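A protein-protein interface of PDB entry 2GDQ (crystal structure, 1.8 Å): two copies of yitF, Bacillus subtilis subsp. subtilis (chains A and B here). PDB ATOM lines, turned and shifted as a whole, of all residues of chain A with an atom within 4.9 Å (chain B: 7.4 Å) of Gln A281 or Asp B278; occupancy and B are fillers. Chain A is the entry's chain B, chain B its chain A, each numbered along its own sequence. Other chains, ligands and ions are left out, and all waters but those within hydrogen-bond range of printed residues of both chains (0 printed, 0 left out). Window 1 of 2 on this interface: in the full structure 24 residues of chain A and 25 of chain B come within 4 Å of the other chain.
NE of Arg A284 is in hydrogen-bond range of O of Pro A312. The backbone carbonyl oxygen of Glu B275 sits at hydrogen-bond distance from the side-chain sulfur of Cys B279 (3.4 Å).
Gln B281 touches Asp A278. OD2 of Asp B278 touches CG of Gln A281, 3.5 Å away. CD1 of Leu A282 touches CD1 of Leu B282 (3.7 Å). Tyr A285 touches Pro B248 (CZ to CG, 3.4 Å). Tyr A285 touches Glu B275. Arg B83 touches Pro A312.
OD2 of Asp B278 lies within hydrogen-bond range of OH of Tyr A285 (2.6 Å). The side-chain hydroxyl of Tyr B285 lies within hydrogen-bond range of the side-chain carboxylate of Asp A278 (2.7 Å).
Of the 11 printed residues of chain A, 5 touch a printed residue of chain B. Printed residues of chain A that touch a printed residue of chain B: Asp A278, Gln A281, Leu A282, Tyr A285 and Pro A312. Of the 21 printed residues of chain B, 7 touch a printed residue of chain A. Hydrophobic or aromatic side chains of chain B within 4 Å of the printed part of chain A: Pro B248, Leu B282 and Tyr B285. Among the printed residues, 8 pairs touch across the chains. Among the printed residues, no Asp or Glu carboxylate lies within 4 Å of a Lys or Arg side-chain nitrogen of the other chain.
Asp B278 touches just these residues of chain A: Gln A281 (3.5 Å) and Tyr A285 (2.6 Å). Of the printed residues of chain A, Gln B281 touches Asp A278 (3.6 Å). Printed residues of chain B within 4 Å of Pro A312: Arg B83 (3.4 Å). Of the printed residues of chain A, Glu B275 touches Tyr A285. Printed residues of chain A within 4 Å of Tyr B285: Asp A278. Leu A311 touches none of the printed residues of chain B. The nearest printed residue of chain A that does not touch Gln B281 is Leu A282 (7.3 Å).
Asp A278 touches Gln B281, and with the chains exchanged Gln A281 touches Asp B278. Asp A278 touches Tyr B285, and with the chains exchanged Tyr A285 touches Asp B278. Leu A282 touches its own counterpart, Leu B282. 9 positions are printed for both chains. Of the 8 pairs that touch across the chains among the printed residues, 5 have their exchanged pair printed and touching as well.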
ATOM      1  N   ARG A 277      11.942  23.461  -6.619  1.00  0.00           N
ATOM      2  CA  ARG A 277      12.597  23.023  -5.383  1.00  0.00           C
ATOM      3  C   ARG A 277      12.624  21.486  -5.271  1.00  0.00           C
ATOM      4  O   ARG A 277      13.626  20.930  -4.838  1.00  0.00           O
ATOM      5  CB  ARG A 277      11.960  23.657  -4.137  1.00  0.00           C
ATOM      6  CG  ARG A 277      12.094  25.186  -4.097  1.00  0.00           C
ATOM      7  CD  ARG A 277      11.689  25.754  -2.714  1.00  0.00           C
ATOM      8  NE  ARG A 277      12.626  25.283  -1.677  1.00  0.00           N
ATOM      9  CZ  ARG A 277      12.278  24.655  -0.559  1.00  0.00           C
ATOM     10  NH1 ARG A 277      10.991  24.472  -0.264  1.00  0.00           N
ATOM     11  NH2 ARG A 277      13.225  24.275   0.306  1.00  0.00           N
ATOM     12  N   ASP A 278      11.562  20.816  -5.732  1.00  0.00           N
ATOM     13  CA  ASP A 278      11.520  19.338  -5.780  1.00  0.00           C
ATOM     14  C   ASP A 278      12.589  18.736  -6.705  1.00  0.00           C
ATOM     15  O   ASP A 278      13.105  17.656  -6.415  1.00  0.00           O
ATOM     16  CB  ASP A 278      10.131  18.835  -6.212  1.00  0.00           C
ATOM     17  CG  ASP A 278       9.068  18.952  -5.093  1.00  0.00           C
ATOM     18  OD1 ASP A 278       9.410  19.170  -3.915  1.00  0.00           O
ATOM     19  OD2 ASP A 278       7.875  18.820  -5.419  1.00  0.00           O
ATOM     20  N   CYS A 279      12.872  19.396  -7.821  1.00  0.00           N
ATOM     21  CA  CYS A 279      13.991  19.011  -8.709  1.00  0.00           C
ATOM     22  C   CYS A 279      15.328  19.056  -7.986  1.00  0.00           C
ATOM     23  O   CYS A 279      16.142  18.147  -8.132  1.00  0.00           O
ATOM     24  CB  CYS A 279      14.060  19.916  -9.947  1.00  0.00           C
ATOM     25  SG  CYS A 279      12.699  19.723 -11.121  1.00  0.00           S
ATOM     26  N   LEU A 280      15.549  20.129  -7.223  1.00  0.00           N
ATOM     27  CA  LEU A 280      16.781  20.282  -6.448  1.00  0.00           C
ATOM     28  C   LEU A 280      16.904  19.173  -5.395  1.00  0.00           C
ATOM     29  O   LEU A 280      17.969  18.600  -5.240  1.00  0.00           O
ATOM     30  CB  LEU A 280      16.891  21.686  -5.783  1.00  0.00           C
ATOM     31  CG  LEU A 280      16.827  22.914  -6.720  1.00  0.00           C
ATOM     32  CD1 LEU A 280      17.038  24.223  -5.923  1.00  0.00           C
ATOM     33  CD2 LEU A 280      17.817  22.832  -7.877  1.00  0.00           C
ATOM     34  N   GLN A 281      15.816  18.905  -4.668  1.00  0.00           N
ATOM     35  CA  GLN A 281      15.846  17.886  -3.630  1.00  0.00           C
ATOM     36  C   GLN A 281      16.042  16.519  -4.273  1.00  0.00           C
ATOM     37  O   GLN A 281      16.782  15.690  -3.730  1.00  0.00           O
ATOM     38  CB  GLN A 281      14.595  17.899  -2.741  1.00  0.00           C
ATOM     39  CG  GLN A 281      14.915  17.794  -1.212  1.00  0.00           C
ATOM     40  CD  GLN A 281      15.852  18.900  -0.684  1.00  0.00           C
ATOM     41  OE1 GLN A 281      16.846  18.623   0.009  1.00  0.00           O
ATOM     42  NE2 GLN A 281      15.540  20.142  -1.005  1.00  0.00           N
ATOM     43  N   LEU A 282      15.384  16.295  -5.412  1.00  0.00           N
ATOM     44  CA  LEU A 282      15.496  15.011  -6.115  1.00  0.00           C
ATOM     45  C   LEU A 282      16.977  14.741  -6.412  1.00  0.00           C
ATOM     46  O   LEU A 282      17.506  13.632  -6.199  1.00  0.00           O
ATOM     47  CB  LEU A 282      14.678  15.017  -7.404  1.00  0.00           C
ATOM     48  CG  LEU A 282      14.784  13.770  -8.287  1.00  0.00           C
ATOM     49  CD1 LEU A 282      14.010  12.557  -7.638  1.00  0.00           C
ATOM     50  CD2 LEU A 282      14.203  14.098  -9.679  1.00  0.00           C
ATOM     51  N   ALA A 283      17.660  15.777  -6.849  1.00  0.00           N
ATOM     52  CA  ALA A 283      19.072  15.642  -7.187  1.00  0.00           C
ATOM     53  C   ALA A 283      19.840  15.221  -5.933  1.00  0.00           C
ATOM     54  O   ALA A 283      20.607  14.257  -5.988  1.00  0.00           O
ATOM     55  CB  ALA A 283      19.633  16.940  -7.813  1.00  0.00           C
ATOM     56  N   ARG A 284      19.592  15.903  -4.803  1.00  0.00           N
ATOM     57  CA  ARG A 284      20.254  15.582  -3.539  1.00  0.00           C
ATOM     58  C   ARG A 284      20.008  14.122  -3.167  1.00  0.00           C
ATOM     59  O   ARG A 284      20.934  13.440  -2.742  1.00  0.00           O
ATOM     60  CB  ARG A 284      19.793  16.507  -2.395  1.00  0.00           C
ATOM     61  CG  ARG A 284      20.451  17.934  -2.431  1.00  0.00           C
ATOM     62  CD  ARG A 284      21.969  17.928  -2.086  1.00  0.00           C
ATOM     63  NE  ARG A 284      22.520  19.284  -2.181  1.00  0.00           N
ATOM     64  CZ  ARG A 284      22.932  19.886  -3.285  1.00  0.00           C
ATOM     65  NH1 ARG A 284      23.006  19.220  -4.462  1.00  0.00           N
ATOM     66  NH2 ARG A 284      23.369  21.141  -3.186  1.00  0.00           N
ATOM     67  N   TYR A 285      18.761  13.659  -3.338  1.00  0.00           N
ATOM     68  CA  TYR A 285      18.409  12.290  -2.965  1.00  0.00           C
ATOM     69  C   TYR A 285      19.060  11.257  -3.858  1.00  0.00           C
ATOM     70  O   TYR A 285      19.365  10.159  -3.410  1.00  0.00           O
ATOM     71  CB  TYR A 285      16.900  12.102  -2.924  1.00  0.00           C
ATOM     72  CG  TYR A 285      16.257  12.881  -1.782  1.00  0.00           C
ATOM     73  CD1 TYR A 285      16.817  12.858  -0.508  1.00  0.00           C
ATOM     74  CD2 TYR A 285      15.113  13.640  -1.984  1.00  0.00           C
ATOM     75  CE1 TYR A 285      16.250  13.567   0.569  1.00  0.00           C
ATOM     76  CE2 TYR A 285      14.523  14.372  -0.897  1.00  0.00           C
ATOM     77  CZ  TYR A 285      15.113  14.325   0.361  1.00  0.00           C
ATOM     78  OH  TYR A 285      14.583  15.026   1.424  1.00  0.00           O
ATOM     79  N   LEU A 311      19.054  24.948   0.179  1.00  0.00           N
ATOM     80  CA  LEU A 311      19.470  23.602  -0.226  1.00  0.00           C
ATOM     81  C   LEU A 311      20.648  23.119   0.648  1.00  0.00           C
ATOM     82  O   LEU A 311      21.614  23.863   0.867  1.00  0.00           O
ATOM     83  CB  LEU A 311      19.816  23.552  -1.730  1.00  0.00           C
ATOM     84  CG  LEU A 311      19.872  22.226  -2.497  1.00  0.00           C
ATOM     85  CD1 LEU A 311      18.502  21.531  -2.623  1.00  0.00           C
ATOM     86  CD2 LEU A 311      20.468  22.468  -3.899  1.00  0.00           C
ATOM     87  N   PRO A 312      20.575  21.868   1.139  1.00  0.00           N
ATOM     88  CA  PRO A 312      21.689  21.340   1.923  1.00  0.00           C
ATOM     89  C   PRO A 312      22.967  21.210   1.071  1.00  0.00           C
ATOM     90  O   PRO A 312      22.866  21.156  -0.154  1.00  0.00           O
ATOM     91  CB  PRO A 312      21.174  19.970   2.378  1.00  0.00           C
ATOM     92  CG  PRO A 312      20.181  19.579   1.356  1.00  0.00           C
ATOM     93  CD  PRO A 312      19.517  20.865   0.938  1.00  0.00           C
ATOM     94  N   LEU B  79      15.020  23.788   8.723  1.00  0.00           N
ATOM     95  CA  LEU B  79      15.762  22.828   7.862  1.00  0.00           C
ATOM     96  C   LEU B  79      17.116  22.514   8.491  1.00  0.00           C
ATOM     97  O   LEU B  79      17.493  21.331   8.674  1.00  0.00           O
ATOM     98  CB  LEU B  79      15.956  23.378   6.440  1.00  0.00           C
ATOM     99  CG  LEU B  79      14.665  23.656   5.626  1.00  0.00           C
ATOM    100  CD1 LEU B  79      14.998  24.139   4.235  1.00  0.00           C
ATOM    101  CD2 LEU B  79      13.761  22.454   5.552  1.00  0.00           C
ATOM    102  N   ARG B  83      18.403  18.969  10.329  1.00  0.00           N
ATOM    103  CA  ARG B  83      19.540  18.322   9.704  1.00  0.00           C
ATOM    104  C   ARG B  83      20.702  18.081  10.707  1.00  0.00           C
ATOM    105  O   ARG B  83      21.325  17.024  10.677  1.00  0.00           O
ATOM    106  CB  ARG B  83      19.978  19.136   8.474  1.00  0.00           C
ATOM    107  CG  ARG B  83      21.401  18.893   8.073  1.00  0.00           C
ATOM    108  CD  ARG B  83      21.687  19.538   6.748  1.00  0.00           C
ATOM    109  NE  ARG B  83      21.347  18.599   5.691  1.00  0.00           N
ATOM    110  CZ  ARG B  83      22.258  17.908   5.019  1.00  0.00           C
ATOM    111  NH1 ARG B  83      21.884  17.063   4.062  1.00  0.00           N
ATOM    112  NH2 ARG B  83      23.544  18.099   5.283  1.00  0.00           N
ATOM    113  N   GLY B 247      14.719   7.463   4.817  1.00  0.00           N
ATOM    114  CA  GLY B 247      14.543   8.711   4.080  1.00  0.00           C
ATOM    115  C   GLY B 247      14.383   8.472   2.594  1.00  0.00           C
ATOM    116  O   GLY B 247      14.512   7.315   2.133  1.00  0.00           O
ATOM    117  N   PRO B 248      14.072   9.558   1.838  1.00  0.00           N
ATOM    118  CA  PRO B 248      13.858   9.454   0.394  1.00  0.00           C
ATOM    119  C   PRO B 248      15.030   8.786  -0.347  1.00  0.00           C
ATOM    120  O   PRO B 248      14.781   8.016  -1.279  1.00  0.00           O
ATOM    121  CB  PRO B 248      13.640  10.919  -0.051  1.00  0.00           C
ATOM    122  CG  PRO B 248      13.198  11.666   1.234  1.00  0.00           C
ATOM    123  CD  PRO B 248      13.877  10.940   2.349  1.00  0.00           C
ATOM    124  N   TYR B 251      14.511   5.115  -0.590  1.00  0.00           N
ATOM    125  CA  TYR B 251      13.449   4.684  -1.492  1.00  0.00           C
ATOM    126  C   TYR B 251      13.886   4.684  -2.945  1.00  0.00           C
ATOM    127  O   TYR B 251      13.389   3.880  -3.731  1.00  0.00           O
ATOM    128  CB  TYR B 251      12.225   5.597  -1.356  1.00  0.00           C
ATOM    129  CG  TYR B 251      11.414   5.260  -0.126  1.00  0.00           C
ATOM    130  CD1 TYR B 251      11.404   6.129   0.958  1.00  0.00           C
ATOM    131  CD2 TYR B 251      10.696   4.049  -0.028  1.00  0.00           C
ATOM    132  CE1 TYR B 251      10.693   5.843   2.095  1.00  0.00           C
ATOM    133  CE2 TYR B 251       9.974   3.749   1.139  1.00  0.00           C
ATOM    134  CZ  TYR B 251       9.985   4.658   2.178  1.00  0.00           C
ATOM    135  OH  TYR B 251       9.322   4.436   3.355  1.00  0.00           O
ATOM    136  N   ILE B 263       4.719   2.633  -1.517  1.00  0.00           N
ATOM    137  CA  ILE B 263       5.646   2.899  -0.415  1.00  0.00           C
ATOM    138  C   ILE B 263       4.930   3.364   0.862  1.00  0.00           C
ATOM    139  O   ILE B 263       3.811   3.951   0.823  1.00  0.00           O
ATOM    140  CB  ILE B 263       6.831   3.856  -0.803  1.00  0.00           C
ATOM    141  CG1 ILE B 263       6.352   5.310  -1.022  1.00  0.00           C
ATOM    142  CG2 ILE B 263       7.636   3.301  -1.987  1.00  0.00           C
ATOM    143  CD1 ILE B 263       7.544   6.278  -1.258  1.00  0.00           C
ATOM    144  N   PRO B 265       6.172   5.249   3.952  1.00  0.00           N
ATOM    145  CA  PRO B 265       7.028   5.979   4.879  1.00  0.00           C
ATOM    146  C   PRO B 265       6.296   6.202   6.203  1.00  0.00           C
ATOM    147  O   PRO B 265       5.042   6.251   6.240  1.00  0.00           O
ATOM    148  CB  PRO B 265       7.282   7.323   4.149  1.00  0.00           C
ATOM    149  CG  PRO B 265       6.099   7.465   3.217  1.00  0.00           C
ATOM    150  CD  PRO B 265       5.777   6.049   2.780  1.00  0.00           C
ATOM    151  N   GLY B 272      12.140  13.537   9.824  1.00  0.00           N
ATOM    152  CA  GLY B 272      11.311  14.709   9.955  1.00  0.00           C
ATOM    153  C   GLY B 272      10.205  14.808   8.951  1.00  0.00           C
ATOM    154  O   GLY B 272      10.142  14.042   7.974  1.00  0.00           O
ATOM    155  N   ILE B 273       9.323  15.761   9.212  1.00  0.00           N
ATOM    156  CA  ILE B 273       8.124  15.969   8.403  1.00  0.00           C
ATOM    157  C   ILE B 273       8.438  16.425   6.978  1.00  0.00           C
ATOM    158  O   ILE B 273       7.664  16.115   6.051  1.00  0.00           O
ATOM    159  CB  ILE B 273       7.103  16.915   9.127  1.00  0.00           C
ATOM    160  CG1 ILE B 273       5.750  16.980   8.384  1.00  0.00           C
ATOM    161  CG2 ILE B 273       7.723  18.296   9.396  1.00  0.00           C
ATOM    162  CD1 ILE B 273       5.149  15.542   8.062  1.00  0.00           C
ATOM    163  N   ASP B 274       9.552  17.147   6.777  1.00  0.00           N
ATOM    164  CA  ASP B 274       9.857  17.667   5.408  1.00  0.00           C
ATOM    165  C   ASP B 274      10.422  16.531   4.557  1.00  0.00           C
ATOM    166  O   ASP B 274      10.062  16.371   3.375  1.00  0.00           O
ATOM    167  CB  ASP B 274      10.793  18.881   5.467  1.00  0.00           C
ATOM    168  CG  ASP B 274      10.190  20.049   6.289  1.00  0.00           C
ATOM    169  OD1 ASP B 274       9.042  20.486   5.990  1.00  0.00           O
ATOM    170  OD2 ASP B 274      10.851  20.504   7.225  1.00  0.00           O
ATOM    171  N   GLU B 275      11.294  15.738   5.154  1.00  0.00           N
ATOM    172  CA  GLU B 275      11.762  14.513   4.512  1.00  0.00           C
ATOM    173  C   GLU B 275      10.607  13.529   4.257  1.00  0.00           C
ATOM    174  O   GLU B 275      10.531  12.918   3.182  1.00  0.00           O
ATOM    175  CB  GLU B 275      12.944  13.891   5.292  1.00  0.00           C
ATOM    176  CG  GLU B 275      14.257  14.703   5.050  1.00  0.00           C
ATOM    177  CD  GLU B 275      15.570  13.913   5.173  1.00  0.00           C
ATOM    178  OE1 GLU B 275      15.618  12.700   4.827  1.00  0.00           O
ATOM    179  OE2 GLU B 275      16.591  14.531   5.599  1.00  0.00           O
ATOM    180  N   PHE B 276       9.687  13.392   5.219  1.00  0.00           N
ATOM    181  CA  PHE B 276       8.489  12.557   4.995  1.00  0.00           C
ATOM    182  C   PHE B 276       7.700  13.020   3.759  1.00  0.00           C
ATOM    183  O   PHE B 276       7.346  12.220   2.914  1.00  0.00           O
ATOM    184  CB  PHE B 276       7.593  12.564   6.224  1.00  0.00           C
ATOM    185  CG  PHE B 276       6.316  11.795   6.064  1.00  0.00           C
ATOM    186  CD1 PHE B 276       6.284  10.437   6.308  1.00  0.00           C
ATOM    187  CD2 PHE B 276       5.122  12.451   5.700  1.00  0.00           C
ATOM    188  CE1 PHE B 276       5.064   9.714   6.160  1.00  0.00           C
ATOM    189  CE2 PHE B 276       3.903  11.757   5.565  1.00  0.00           C
ATOM    190  CZ  PHE B 276       3.875  10.393   5.802  1.00  0.00           C
ATOM    191  N   ARG B 277       7.391  14.310   3.688  1.00  0.00           N
ATOM    192  CA  ARG B 277       6.683  14.850   2.549  1.00  0.00           C
ATOM    193  C   ARG B 277       7.452  14.624   1.232  1.00  0.00           C
ATOM    194  O   ARG B 277       6.827  14.270   0.221  1.00  0.00           O
ATOM    195  CB  ARG B 277       6.379  16.340   2.758  1.00  0.00           C
ATOM    196  CG  ARG B 277       5.353  16.584   3.909  1.00  0.00           C
ATOM    197  CD  ARG B 277       4.886  18.057   3.890  1.00  0.00           C
ATOM    198  NE  ARG B 277       4.103  18.291   2.671  1.00  0.00           N
ATOM    199  CZ  ARG B 277       4.258  19.309   1.827  1.00  0.00           C
ATOM    200  NH1 ARG B 277       5.145  20.276   2.056  1.00  0.00           N
ATOM    201  NH2 ARG B 277       3.479  19.375   0.770  1.00  0.00           N
ATOM    202  N   ASP B 278       8.778  14.774   1.270  1.00  0.00           N
ATOM    203  CA  ASP B 278       9.647  14.410   0.118  1.00  0.00           C
ATOM    204  C   ASP B 278       9.476  12.945  -0.286  1.00  0.00           C
ATOM    205  O   ASP B 278       9.473  12.668  -1.491  1.00  0.00           O
ATOM    206  CB  ASP B 278      11.153  14.733   0.346  1.00  0.00           C
ATOM    207  CG  ASP B 278      11.458  16.257   0.487  1.00  0.00           C
ATOM    208  OD1 ASP B 278      10.663  17.116   0.089  1.00  0.00           O
ATOM    209  OD2 ASP B 278      12.536  16.579   1.002  1.00  0.00           O
ATOM    210  N   CYS B 279       9.338  12.011   0.675  1.00  0.00           N
ATOM    211  CA  CYS B 279       9.011  10.607   0.352  1.00  0.00           C
ATOM    212  C   CYS B 279       7.749  10.452  -0.509  1.00  0.00           C
ATOM    213  O   CYS B 279       7.756   9.723  -1.539  1.00  0.00           O
ATOM    214  CB  CYS B 279       8.891   9.735   1.609  1.00  0.00           C
ATOM    215  SG  CYS B 279      10.410   9.580   2.466  1.00  0.00           S
ATOM    216  N   LEU B 280       6.690  11.164  -0.112  1.00  0.00           N
ATOM    217  CA  LEU B 280       5.428  11.121  -0.845  1.00  0.00           C
ATOM    218  C   LEU B 280       5.573  11.743  -2.219  1.00  0.00           C
ATOM    219  O   LEU B 280       5.054  11.195  -3.180  1.00  0.00           O
ATOM    220  CB  LEU B 280       4.263  11.776  -0.067  1.00  0.00           C
ATOM    221  CG  LEU B 280       3.993  11.352   1.414  1.00  0.00           C
ATOM    222  CD1 LEU B 280       2.882  12.234   2.004  1.00  0.00           C
ATOM    223  CD2 LEU B 280       3.647   9.883   1.652  1.00  0.00           C
ATOM    224  N   GLN B 281       6.230  12.901  -2.309  1.00  0.00           N
ATOM    225  CA  GLN B 281       6.510  13.511  -3.611  1.00  0.00           C
ATOM    226  C   GLN B 281       7.319  12.577  -4.500  1.00  0.00           C
ATOM    227  O   GLN B 281       7.026  12.459  -5.678  1.00  0.00           O
ATOM    228  CB  GLN B 281       7.287  14.815  -3.478  1.00  0.00           C
ATOM    229  CG  GLN B 281       6.507  15.922  -2.810  1.00  0.00           C
ATOM    230  CD  GLN B 281       5.230  16.237  -3.553  1.00  0.00           C
ATOM    231  OE1 GLN B 281       5.236  16.418  -4.774  1.00  0.00           O
ATOM    232  NE2 GLN B 281       4.135  16.290  -2.831  1.00  0.00           N
ATOM    233  N   LEU B 282       8.370  11.981  -3.952  1.00  0.00           N
ATOM    234  CA  LEU B 282       9.220  11.023  -4.703  1.00  0.00           C
ATOM    235  C   LEU B 282       8.378   9.917  -5.328  1.00  0.00           C
ATOM    236  O   LEU B 282       8.535   9.598  -6.505  1.00  0.00           O
ATOM    237  CB  LEU B 282      10.262  10.388  -3.782  1.00  0.00           C
ATOM    238  CG  LEU B 282      11.339   9.500  -4.395  1.00  0.00           C
ATOM    239  CD1 LEU B 282      12.261  10.358  -5.292  1.00  0.00           C
ATOM    240  CD2 LEU B 282      12.142   8.835  -3.260  1.00  0.00           C
ATOM    241  N   ALA B 283       7.501   9.308  -4.531  1.00  0.00           N
ATOM    242  CA  ALA B 283       6.567   8.282  -5.028  1.00  0.00           C
ATOM    243  C   ALA B 283       5.760   8.803  -6.228  1.00  0.00           C
ATOM    244  O   ALA B 283       5.708   8.164  -7.268  1.00  0.00           O
ATOM    245  CB  ALA B 283       5.612   7.793  -3.894  1.00  0.00           C
ATOM    246  N   ARG B 284       5.138   9.964  -6.079  1.00  0.00           N
ATOM    247  CA  ARG B 284       4.407  10.576  -7.199  1.00  0.00           C
ATOM    248  C   ARG B 284       5.237  10.733  -8.476  1.00  0.00           C
ATOM    249  O   ARG B 284       4.744  10.458  -9.568  1.00  0.00           O
ATOM    250  CB  ARG B 284       3.856  11.956  -6.788  1.00  0.00           C
ATOM    251  CG  ARG B 284       2.570  11.905  -5.879  1.00  0.00           C
ATOM    252  CD  ARG B 284       1.344  11.330  -6.602  1.00  0.00           C
ATOM    253  NE  ARG B 284       0.180  11.262  -5.683  1.00  0.00           N
ATOM    254  CZ  ARG B 284      -0.096  10.242  -4.873  1.00  0.00           C
ATOM    255  NH1 ARG B 284       0.684   9.157  -4.858  1.00  0.00           N
ATOM    256  NH2 ARG B 284      -1.164  10.300  -4.076  1.00  0.00           N
ATOM    257  N   TYR B 285       6.470  11.228  -8.334  1.00  0.00           N
ATOM    258  CA  TYR B 285       7.358  11.426  -9.492  1.00  0.00           C
ATOM    259  C   TYR B 285       7.814  10.106 -10.142  1.00  0.00           C
ATOM    260  O   TYR B 285       8.120  10.053 -11.363  1.00  0.00           O
ATOM    261  CB  TYR B 285       8.565  12.297  -9.114  1.00  0.00           C
ATOM    262  CG  TYR B 285       8.189  13.685  -8.740  1.00  0.00           C
ATOM    263  CD1 TYR B 285       7.286  14.412  -9.516  1.00  0.00           C
ATOM    264  CD2 TYR B 285       8.759  14.316  -7.616  1.00  0.00           C
ATOM    265  CE1 TYR B 285       6.918  15.733  -9.168  1.00  0.00           C
ATOM    266  CE2 TYR B 285       8.374  15.629  -7.259  1.00  0.00           C
ATOM    267  CZ  TYR B 285       7.463  16.327  -8.046  1.00  0.00           C
ATOM    268  OH  TYR B 285       7.090  17.630  -7.720  1.00  0.00           O
